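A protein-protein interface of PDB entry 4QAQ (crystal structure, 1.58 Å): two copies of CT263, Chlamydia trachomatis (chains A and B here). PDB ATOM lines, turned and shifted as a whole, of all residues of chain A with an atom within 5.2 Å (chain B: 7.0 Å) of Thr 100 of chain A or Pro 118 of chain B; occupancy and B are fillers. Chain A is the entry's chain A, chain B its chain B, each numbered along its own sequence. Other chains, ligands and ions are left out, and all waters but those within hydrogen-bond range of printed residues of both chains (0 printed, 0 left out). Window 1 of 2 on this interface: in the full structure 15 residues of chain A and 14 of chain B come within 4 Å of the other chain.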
ATOM      1  N   GLU A  98     -11.236 -35.458   8.400  1.00  0.00           N
ATOM      2  CA  GLU A  98     -10.923 -34.068   8.722  1.00  0.00           C
ATOM      3  C   GLU A  98     -12.182 -33.458   9.295  1.00  0.00           C
ATOM      4  O   GLU A  98     -13.260 -33.594   8.711  1.00  0.00           O
ATOM      5  CB  GLU A  98     -10.459 -33.266   7.503  1.00  0.00           C
ATOM      6  CG  GLU A  98     -10.117 -31.800   7.783  1.00  0.00           C
ATOM      7  CD  GLU A  98      -8.772 -31.623   8.484  1.00  0.00           C
ATOM      8  OE1 GLU A  98      -7.798 -32.298   8.087  1.00  0.00           O
ATOM      9  OE2 GLU A  98      -8.679 -30.809   9.425  1.00  0.00           O
ATOM     10  N   LEU A  99     -12.044 -32.759  10.414  1.00  0.00           N
ATOM     11  CA  LEU A  99     -13.153 -32.085  11.062  1.00  0.00           C
ATOM     12  C   LEU A  99     -12.870 -30.589  11.179  1.00  0.00           C
ATOM     13  O   LEU A  99     -11.791 -30.182  11.646  1.00  0.00           O
ATOM     14  CB  LEU A  99     -13.389 -32.701  12.447  1.00  0.00           C
ATOM     15  CG  LEU A  99     -14.401 -32.002  13.355  1.00  0.00           C
ATOM     16  CD1 LEU A  99     -15.819 -32.082  12.789  1.00  0.00           C
ATOM     17  CD2 LEU A  99     -14.341 -32.585  14.779  1.00  0.00           C
ATOM     18  N   THR A 100     -13.866 -29.771  10.789  1.00  0.00           N
ATOM     19  CA  THR A 100     -13.905 -28.330  10.985  1.00  0.00           C
ATOM     20  C   THR A 100     -14.869 -28.017  12.125  1.00  0.00           C
ATOM     21  O   THR A 100     -16.092 -28.015  11.918  1.00  0.00           O
ATOM     22  CB  THR A 100     -14.342 -27.619   9.705  1.00  0.00           C
ATOM     23  OG1 THR A 100     -13.431 -27.956   8.635  1.00  0.00           O
ATOM     24  CG2 THR A 100     -14.391 -26.098   9.878  1.00  0.00           C
ATOM     25  N   PRO A 101     -14.377 -27.704  13.319  1.00  0.00           N
ATOM     26  CA  PRO A 101     -15.288 -27.542  14.471  1.00  0.00           C
ATOM     27  C   PRO A 101     -16.277 -26.395  14.342  1.00  0.00           C
ATOM     28  O   PRO A 101     -17.363 -26.475  14.931  1.00  0.00           O
ATOM     29  CB  PRO A 101     -14.322 -27.307  15.629  1.00  0.00           C
ATOM     30  CG  PRO A 101     -12.999 -27.820  15.183  1.00  0.00           C
ATOM     31  CD  PRO A 101     -12.956 -27.656  13.707  1.00  0.00           C
ATOM     32  N   THR A 102     -15.945 -25.310  13.642  1.00  0.00           N
ATOM     33  CA  THR A 102     -16.863 -24.176  13.591  1.00  0.00           C
ATOM     34  C   THR A 102     -18.096 -24.458  12.737  1.00  0.00           C
ATOM     35  O   THR A 102     -19.092 -23.743  12.868  1.00  0.00           O
ATOM     36  CB  THR A 102     -16.178 -22.899  13.069  1.00  0.00           C
ATOM     37  OG1 THR A 102     -15.523 -23.161  11.799  1.00  0.00           O
ATOM     38  CG2 THR A 102     -15.182 -22.342  14.112  1.00  0.00           C
ATOM     39  N   THR A 103     -18.054 -25.467  11.856  1.00  0.00           N
ATOM     40  CA  THR A 103     -19.194 -25.806  11.020  1.00  0.00           C
ATOM     41  C   THR A 103     -19.681 -27.235  11.219  1.00  0.00           C
ATOM     42  O   THR A 103     -20.788 -27.557  10.747  1.00  0.00           O
ATOM     43  CB  THR A 103     -18.829 -25.638   9.533  1.00  0.00           C
ATOM     44  OG1 THR A 103     -17.744 -26.506   9.276  1.00  0.00           O
ATOM     45  CG2 THR A 103     -18.419 -24.210   9.223  1.00  0.00           C
ATOM     46  N   SER A 104     -18.884 -28.085  11.853  1.00  0.00           N
ATOM     47  CA  SER A 104     -19.084 -29.522  12.017  1.00  0.00           C
ATOM     48  C   SER A 104     -19.004 -30.273  10.701  1.00  0.00           C
ATOM     49  O   SER A 104     -19.307 -31.477  10.662  1.00  0.00           O
ATOM     50  CB  SER A 104     -20.419 -29.846  12.696  1.00  0.00           C
ATOM     51  OG  SER A 104     -20.414 -29.360  14.026  1.00  0.00           O
ATOM     52  N   VAL A 105     -18.567 -29.623   9.621  1.00  0.00           N
ATOM     53  CA  VAL A 105     -18.412 -30.340   8.359  1.00  0.00           C
ATOM     54  C   VAL A 105     -17.181 -31.235   8.413  1.00  0.00           C
ATOM     55  O   VAL A 105     -16.133 -30.864   8.966  1.00  0.00           O
ATOM     56  CB  VAL A 105     -18.344 -29.335   7.200  1.00  0.00           C
ATOM     57  CG1 VAL A 105     -18.175 -30.046   5.826  1.00  0.00           C
ATOM     58  CG2 VAL A 105     -19.579 -28.517   7.169  1.00  0.00           C
ATOM     59  N   LYS B  89     -12.398 -15.538   8.362  1.00  0.00           N
ATOM     60  CA  LYS B  89     -11.922 -16.906   8.234  1.00  0.00           C
ATOM     61  C   LYS B  89     -12.178 -17.426   6.823  1.00  0.00           C
ATOM     62  O   LYS B  89     -13.282 -17.292   6.294  1.00  0.00           O
ATOM     63  CB  LYS B  89     -12.601 -17.788   9.272  1.00  0.00           C
ATOM     64  CG  LYS B  89     -12.059 -19.198   9.321  1.00  0.00           C
ATOM     65  CD  LYS B  89     -12.612 -19.904  10.541  1.00  0.00           C
ATOM     66  CE  LYS B  89     -12.106 -21.310  10.690  1.00  0.00           C
ATOM     67  NZ  LYS B  89     -10.685 -21.327  11.138  1.00  0.00           N
ATOM     68  N   THR B  90     -11.152 -18.003   6.195  1.00  0.00           N
ATOM     69  CA  THR B  90     -11.272 -18.506   4.838  1.00  0.00           C
ATOM     70  C   THR B  90     -11.667 -19.980   4.848  1.00  0.00           C
ATOM     71  O   THR B  90     -10.956 -20.820   5.418  1.00  0.00           O
ATOM     72  CB  THR B  90      -9.951 -18.332   4.115  1.00  0.00           C
ATOM     73  OG1 THR B  90      -9.515 -16.968   4.248  1.00  0.00           O
ATOM     74  CG2 THR B  90     -10.087 -18.726   2.673  1.00  0.00           C
ATOM     75  N   TYR B  91     -12.779 -20.292   4.196  1.00  0.00           N
ATOM     76  CA  TYR B  91     -13.309 -21.639   4.081  1.00  0.00           C
ATOM     77  C   TYR B  91     -13.255 -22.117   2.633  1.00  0.00           C
ATOM     78  O   TYR B  91     -13.246 -21.307   1.700  1.00  0.00           O
ATOM     79  CB  TYR B  91     -14.774 -21.675   4.542  1.00  0.00           C
ATOM     80  CG  TYR B  91     -14.993 -21.496   6.018  1.00  0.00           C
ATOM     81  CD1 TYR B  91     -15.152 -20.234   6.558  1.00  0.00           C
ATOM     82  CD2 TYR B  91     -15.069 -22.592   6.881  1.00  0.00           C
ATOM     83  CE1 TYR B  91     -15.359 -20.066   7.901  1.00  0.00           C
ATOM     84  CE2 TYR B  91     -15.270 -22.425   8.210  1.00  0.00           C
ATOM     85  CZ  TYR B  91     -15.406 -21.161   8.713  1.00  0.00           C
ATOM     86  OH  TYR B  91     -15.659 -20.992  10.056  1.00  0.00           O
ATOM     87  N   THR B  92     -13.200 -23.434   2.454  1.00  0.00           N
ATOM     88  CA  THR B  92     -13.502 -24.059   1.179  1.00  0.00           C
ATOM     89  C   THR B  92     -14.854 -24.752   1.307  1.00  0.00           C
ATOM     90  O   THR B  92     -15.286 -25.115   2.398  1.00  0.00           O
ATOM     91  CB  THR B  92     -12.392 -25.025   0.753  1.00  0.00           C
ATOM     92  OG1 THR B  92     -12.629 -25.467  -0.600  1.00  0.00           O
ATOM     93  CG2 THR B  92     -12.317 -26.222   1.628  1.00  0.00           C
ATOM     94  N   ILE B  93     -15.546 -24.863   0.195  1.00  0.00           N
ATOM     95  CA  ILE B  93     -16.939 -25.302   0.165  1.00  0.00           C
ATOM     96  C   ILE B  93     -17.039 -26.755  -0.268  1.00  0.00           C
ATOM     97  O   ILE B  93     -16.371 -27.184  -1.221  1.00  0.00           O
ATOM     98  CB  ILE B  93     -17.753 -24.389  -0.776  1.00  0.00           C
ATOM     99  CG1 ILE B  93     -17.642 -22.925  -0.334  1.00  0.00           C
ATOM    100  CG2 ILE B  93     -19.196 -24.836  -0.839  1.00  0.00           C
ATOM    101  CD1 ILE B  93     -18.066 -22.686   1.161  1.00  0.00           C
ATOM    102  N   THR B  94     -17.864 -27.528   0.438  1.00  0.00           N
ATOM    103  CA  THR B  94     -18.106 -28.934   0.137  1.00  0.00           C
ATOM    104  C   THR B  94     -19.383 -29.166  -0.662  1.00  0.00           C
ATOM    105  O   THR B  94     -19.439 -30.106  -1.459  1.00  0.00           O
ATOM    106  CB  THR B  94     -18.186 -29.759   1.429  1.00  0.00           C
ATOM    107  OG1 THR B  94     -19.225 -29.230   2.263  1.00  0.00           O
ATOM    108  CG2 THR B  94     -16.855 -29.735   2.163  1.00  0.00           C
ATOM    109  N   ILE B 114     -10.779 -27.470  -1.665  1.00  0.00           N
ATOM    110  CA  ILE B 114      -9.360 -27.134  -1.745  1.00  0.00           C
ATOM    111  C   ILE B 114      -8.668 -27.679  -0.504  1.00  0.00           C
ATOM    112  O   ILE B 114      -9.146 -27.430   0.616  1.00  0.00           O
ATOM    113  CB  ILE B 114      -9.182 -25.616  -1.858  1.00  0.00           C
ATOM    114  CG1 ILE B 114      -9.815 -25.079  -3.149  1.00  0.00           C
ATOM    115  CG2 ILE B 114      -7.709 -25.187  -1.769  1.00  0.00           C
ATOM    116  CD1 ILE B 114      -9.143 -25.540  -4.430  1.00  0.00           C
ATOM    117  N   PRO B 115      -7.532 -28.358  -0.639  1.00  0.00           N
ATOM    118  CA  PRO B 115      -6.873 -28.920   0.539  1.00  0.00           C
ATOM    119  C   PRO B 115      -6.431 -27.864   1.527  1.00  0.00           C
ATOM    120  O   PRO B 115      -6.123 -26.719   1.174  1.00  0.00           O
ATOM    121  CB  PRO B 115      -5.659 -29.653  -0.043  1.00  0.00           C
ATOM    122  CG  PRO B 115      -5.926 -29.786  -1.481  1.00  0.00           C
ATOM    123  CD  PRO B 115      -6.775 -28.624  -1.867  1.00  0.00           C
ATOM    124  N   ARG B 116      -6.378 -28.290   2.793  1.00  0.00           N
ATOM    125  CA  ARG B 116      -5.797 -27.514   3.885  1.00  0.00           C
ATOM    126  C   ARG B 116      -6.543 -26.213   4.144  1.00  0.00           C
ATOM    127  O   ARG B 116      -5.945 -25.214   4.557  1.00  0.00           O
ATOM    128  CB  ARG B 116      -4.324 -27.235   3.621  1.00  0.00           C
ATOM    129  CG  ARG B 116      -3.554 -27.291   4.896  1.00  0.00           C
ATOM    130  CD  ARG B 116      -2.087 -27.060   4.711  1.00  0.00           C
ATOM    131  NE  ARG B 116      -1.490 -27.006   6.033  1.00  0.00           N
ATOM    132  CZ  ARG B 116      -1.040 -28.066   6.686  1.00  0.00           C
ATOM    133  NH1 ARG B 116      -1.075 -29.269   6.121  1.00  0.00           N
ATOM    134  NH2 ARG B 116      -0.534 -27.915   7.901  1.00  0.00           N
ATOM    135  N   LEU B 117      -7.855 -26.223   3.933  1.00  0.00           N
ATOM    136  CA  LEU B 117      -8.742 -25.138   4.315  1.00  0.00           C
ATOM    137  C   LEU B 117      -9.906 -25.693   5.121  1.00  0.00           C
ATOM    138  O   LEU B 117     -10.353 -26.816   4.883  1.00  0.00           O
ATOM    139  CB  LEU B 117      -9.307 -24.384   3.107  1.00  0.00           C
ATOM    140  CG  LEU B 117      -8.340 -23.448   2.383  1.00  0.00           C
ATOM    141  CD1 LEU B 117      -8.992 -22.903   1.097  1.00  0.00           C
ATOM    142  CD2 LEU B 117      -7.828 -22.329   3.243  1.00  0.00           C
ATOM    143  N   PRO B 118     -10.381 -24.936   6.104  1.00  0.00           N
ATOM    144  CA  PRO B 118     -11.584 -25.346   6.839  1.00  0.00           C
ATOM    145  C   PRO B 118     -12.769 -25.491   5.897  1.00  0.00           C
ATOM    146  O   PRO B 118     -12.872 -24.800   4.890  1.00  0.00           O
ATOM    147  CB  PRO B 118     -11.810 -24.212   7.834  1.00  0.00           C
ATOM    148  CG  PRO B 118     -10.897 -23.148   7.502  1.00  0.00           C
ATOM    149  CD  PRO B 118      -9.866 -23.626   6.517  1.00  0.00           C
ATOM    150  N   LEU B 119     -13.677 -26.390   6.269  1.00  0.00           N
ATOM    151  CA  LEU B 119     -14.751 -26.824   5.385  1.00  0.00           C
ATOM    152  C   LEU B 119     -16.064 -26.163   5.777  1.00  0.00           C
ATOM    153  O   LEU B 119     -16.358 -26.013   6.967  1.00  0.00           O
ATOM    154  CB  LEU B 119     -14.952 -28.323   5.472  1.00  0.00           C
ATOM    155  CG  LEU B 119     -13.763 -29.246   5.272  1.00  0.00           C
ATOM    156  CD1 LEU B 119     -14.140 -30.674   5.628  1.00  0.00           C
ATOM    157  CD2 LEU B 119     -13.321 -29.097   3.827  1.00  0.00           C
ATOM    158  N   ALA B 120     -16.864 -25.812   4.773  1.00  0.00           N
ATOM    159  CA  ALA B 120     -18.191 -25.260   5.044  1.00  0.00           C
ATOM    160  C   ALA B 120     -19.142 -25.585   3.906  1.00  0.00           C
ATOM    161  O   ALA B 120     -18.723 -25.893   2.792  1.00  0.00           O
ATOM    162  CB  ALA B 120     -18.147 -23.763   5.219  1.00  0.00           C
ATOM    163  N   LYS B 162     -14.431 -19.117   0.170  1.00  0.00           N
ATOM    164  CA  LYS B 162     -15.336 -18.104   0.690  1.00  0.00           C
ATOM    165  C   LYS B 162     -14.826 -17.652   2.046  1.00  0.00           C
ATOM    166  O   LYS B 162     -14.632 -18.489   2.931  1.00  0.00           O
ATOM    167  CB  LYS B 162     -16.749 -18.667   0.801  1.00  0.00           C
ATOM    168  CG  LYS B 162     -17.330 -19.077  -0.553  1.00  0.00           C
ATOM    169  CD  LYS B 162     -17.779 -17.888  -1.397  1.00  0.00           C
ATOM    170  CE  LYS B 162     -18.035 -18.331  -2.829  1.00  0.00           C
ATOM    171  NZ  LYS B 162     -18.845 -17.339  -3.583  1.00  0.00           N
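No position is printed for both chains.
Of the 7 pairs that touch across the chains among the printed residues, none has its exchanged pair printed and touching as well.
The side-chain hydroxyl (OG1) of Thr 103 of chain A sits close to the backbone carbonyl oxygen (O) of Thr 100 of chain A, at 3.5 Å.
The backbone NH (N) of Thr 100 of chain A is in hydrogen-bond range of the backbone carbonyl oxygen (O) of Val 105 of chain A (3.1 Å).
The side-chain hydroxyl (OG1) of Thr 103 of chain A sits close to the backbone NH (N) of Val 105 of chain A.
N of Tyr 91 of chain B lies within hydrogen-bond range of O of Lys 162 of chain B (2.9 Å).
The backbone NH (N) of Thr 92 of chain B lies within hydrogen-bond range of the backbone carbonyl oxygen (O) of Pro 118 of chain B (2.8 Å).
N of Thr 94 of chain B is in hydrogen-bond range of O of Ala 120 of chain B, 3.0 Å away.
Along chain A the printed residues that touch a printed residue of chain B span positions 100 to 105.
Hydrophobic or aromatic side chains of chain B that line the printed part of chain A: Tyr 91, Pro 118 and Leu 119.
Among the printed residues, 7 pairs touch across the chains.
Of chain B, only Pro 118 and Leu 119 come within 4 Å of Thr 100 of chain A.
Printed residues of chain B within 4 Å of Thr 103 of chain A: Tyr 91 and Leu 119.
Printed residues of chain B within 4 Å of Val 105 of chain A: Thr 94 and Leu 119.
Thr 90 of chain B touches none of the printed residues of chain A.
Of chain A, only Thr 100 comes within 4 Å of Pro 118 of chain B.
Of the printed residues of chain A, Leu 119 of chain B touches Thr 100, Thr 103 and Val 105.
Ala 120 of chain B touches none of the printed residues of chain A.
The nearest printed residue of chain A that does not touch Pro 118 of chain B is Thr 102 of chain A (5.5 Å).
Among the printed residues, pairs that only touch across the chains: Thr 100 of chain A with Pro 118 of chain B, Val 105 of chain A with Leu 119 of chain B, Thr 103 of chain A with Tyr 91 of chain B and Val 105 of chain A with Thr 94 of chain B.
OG1 of Thr 100 of chain A lies within hydrogen-bond range of N of Leu 119 of chain B (2.8 Å).
The side-chain hydroxyl (OH) of Tyr 91 of chain B lies within hydrogen-bond range of the side-chain hydroxyl (OG1) of Thr 102 of chain A, at 2.8 Å.
The side-chain hydroxyl (OG1) of Thr 103 of chain A lies within hydrogen-bond range of the backbone carbonyl oxygen (O) of Leu 119 of chain B.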
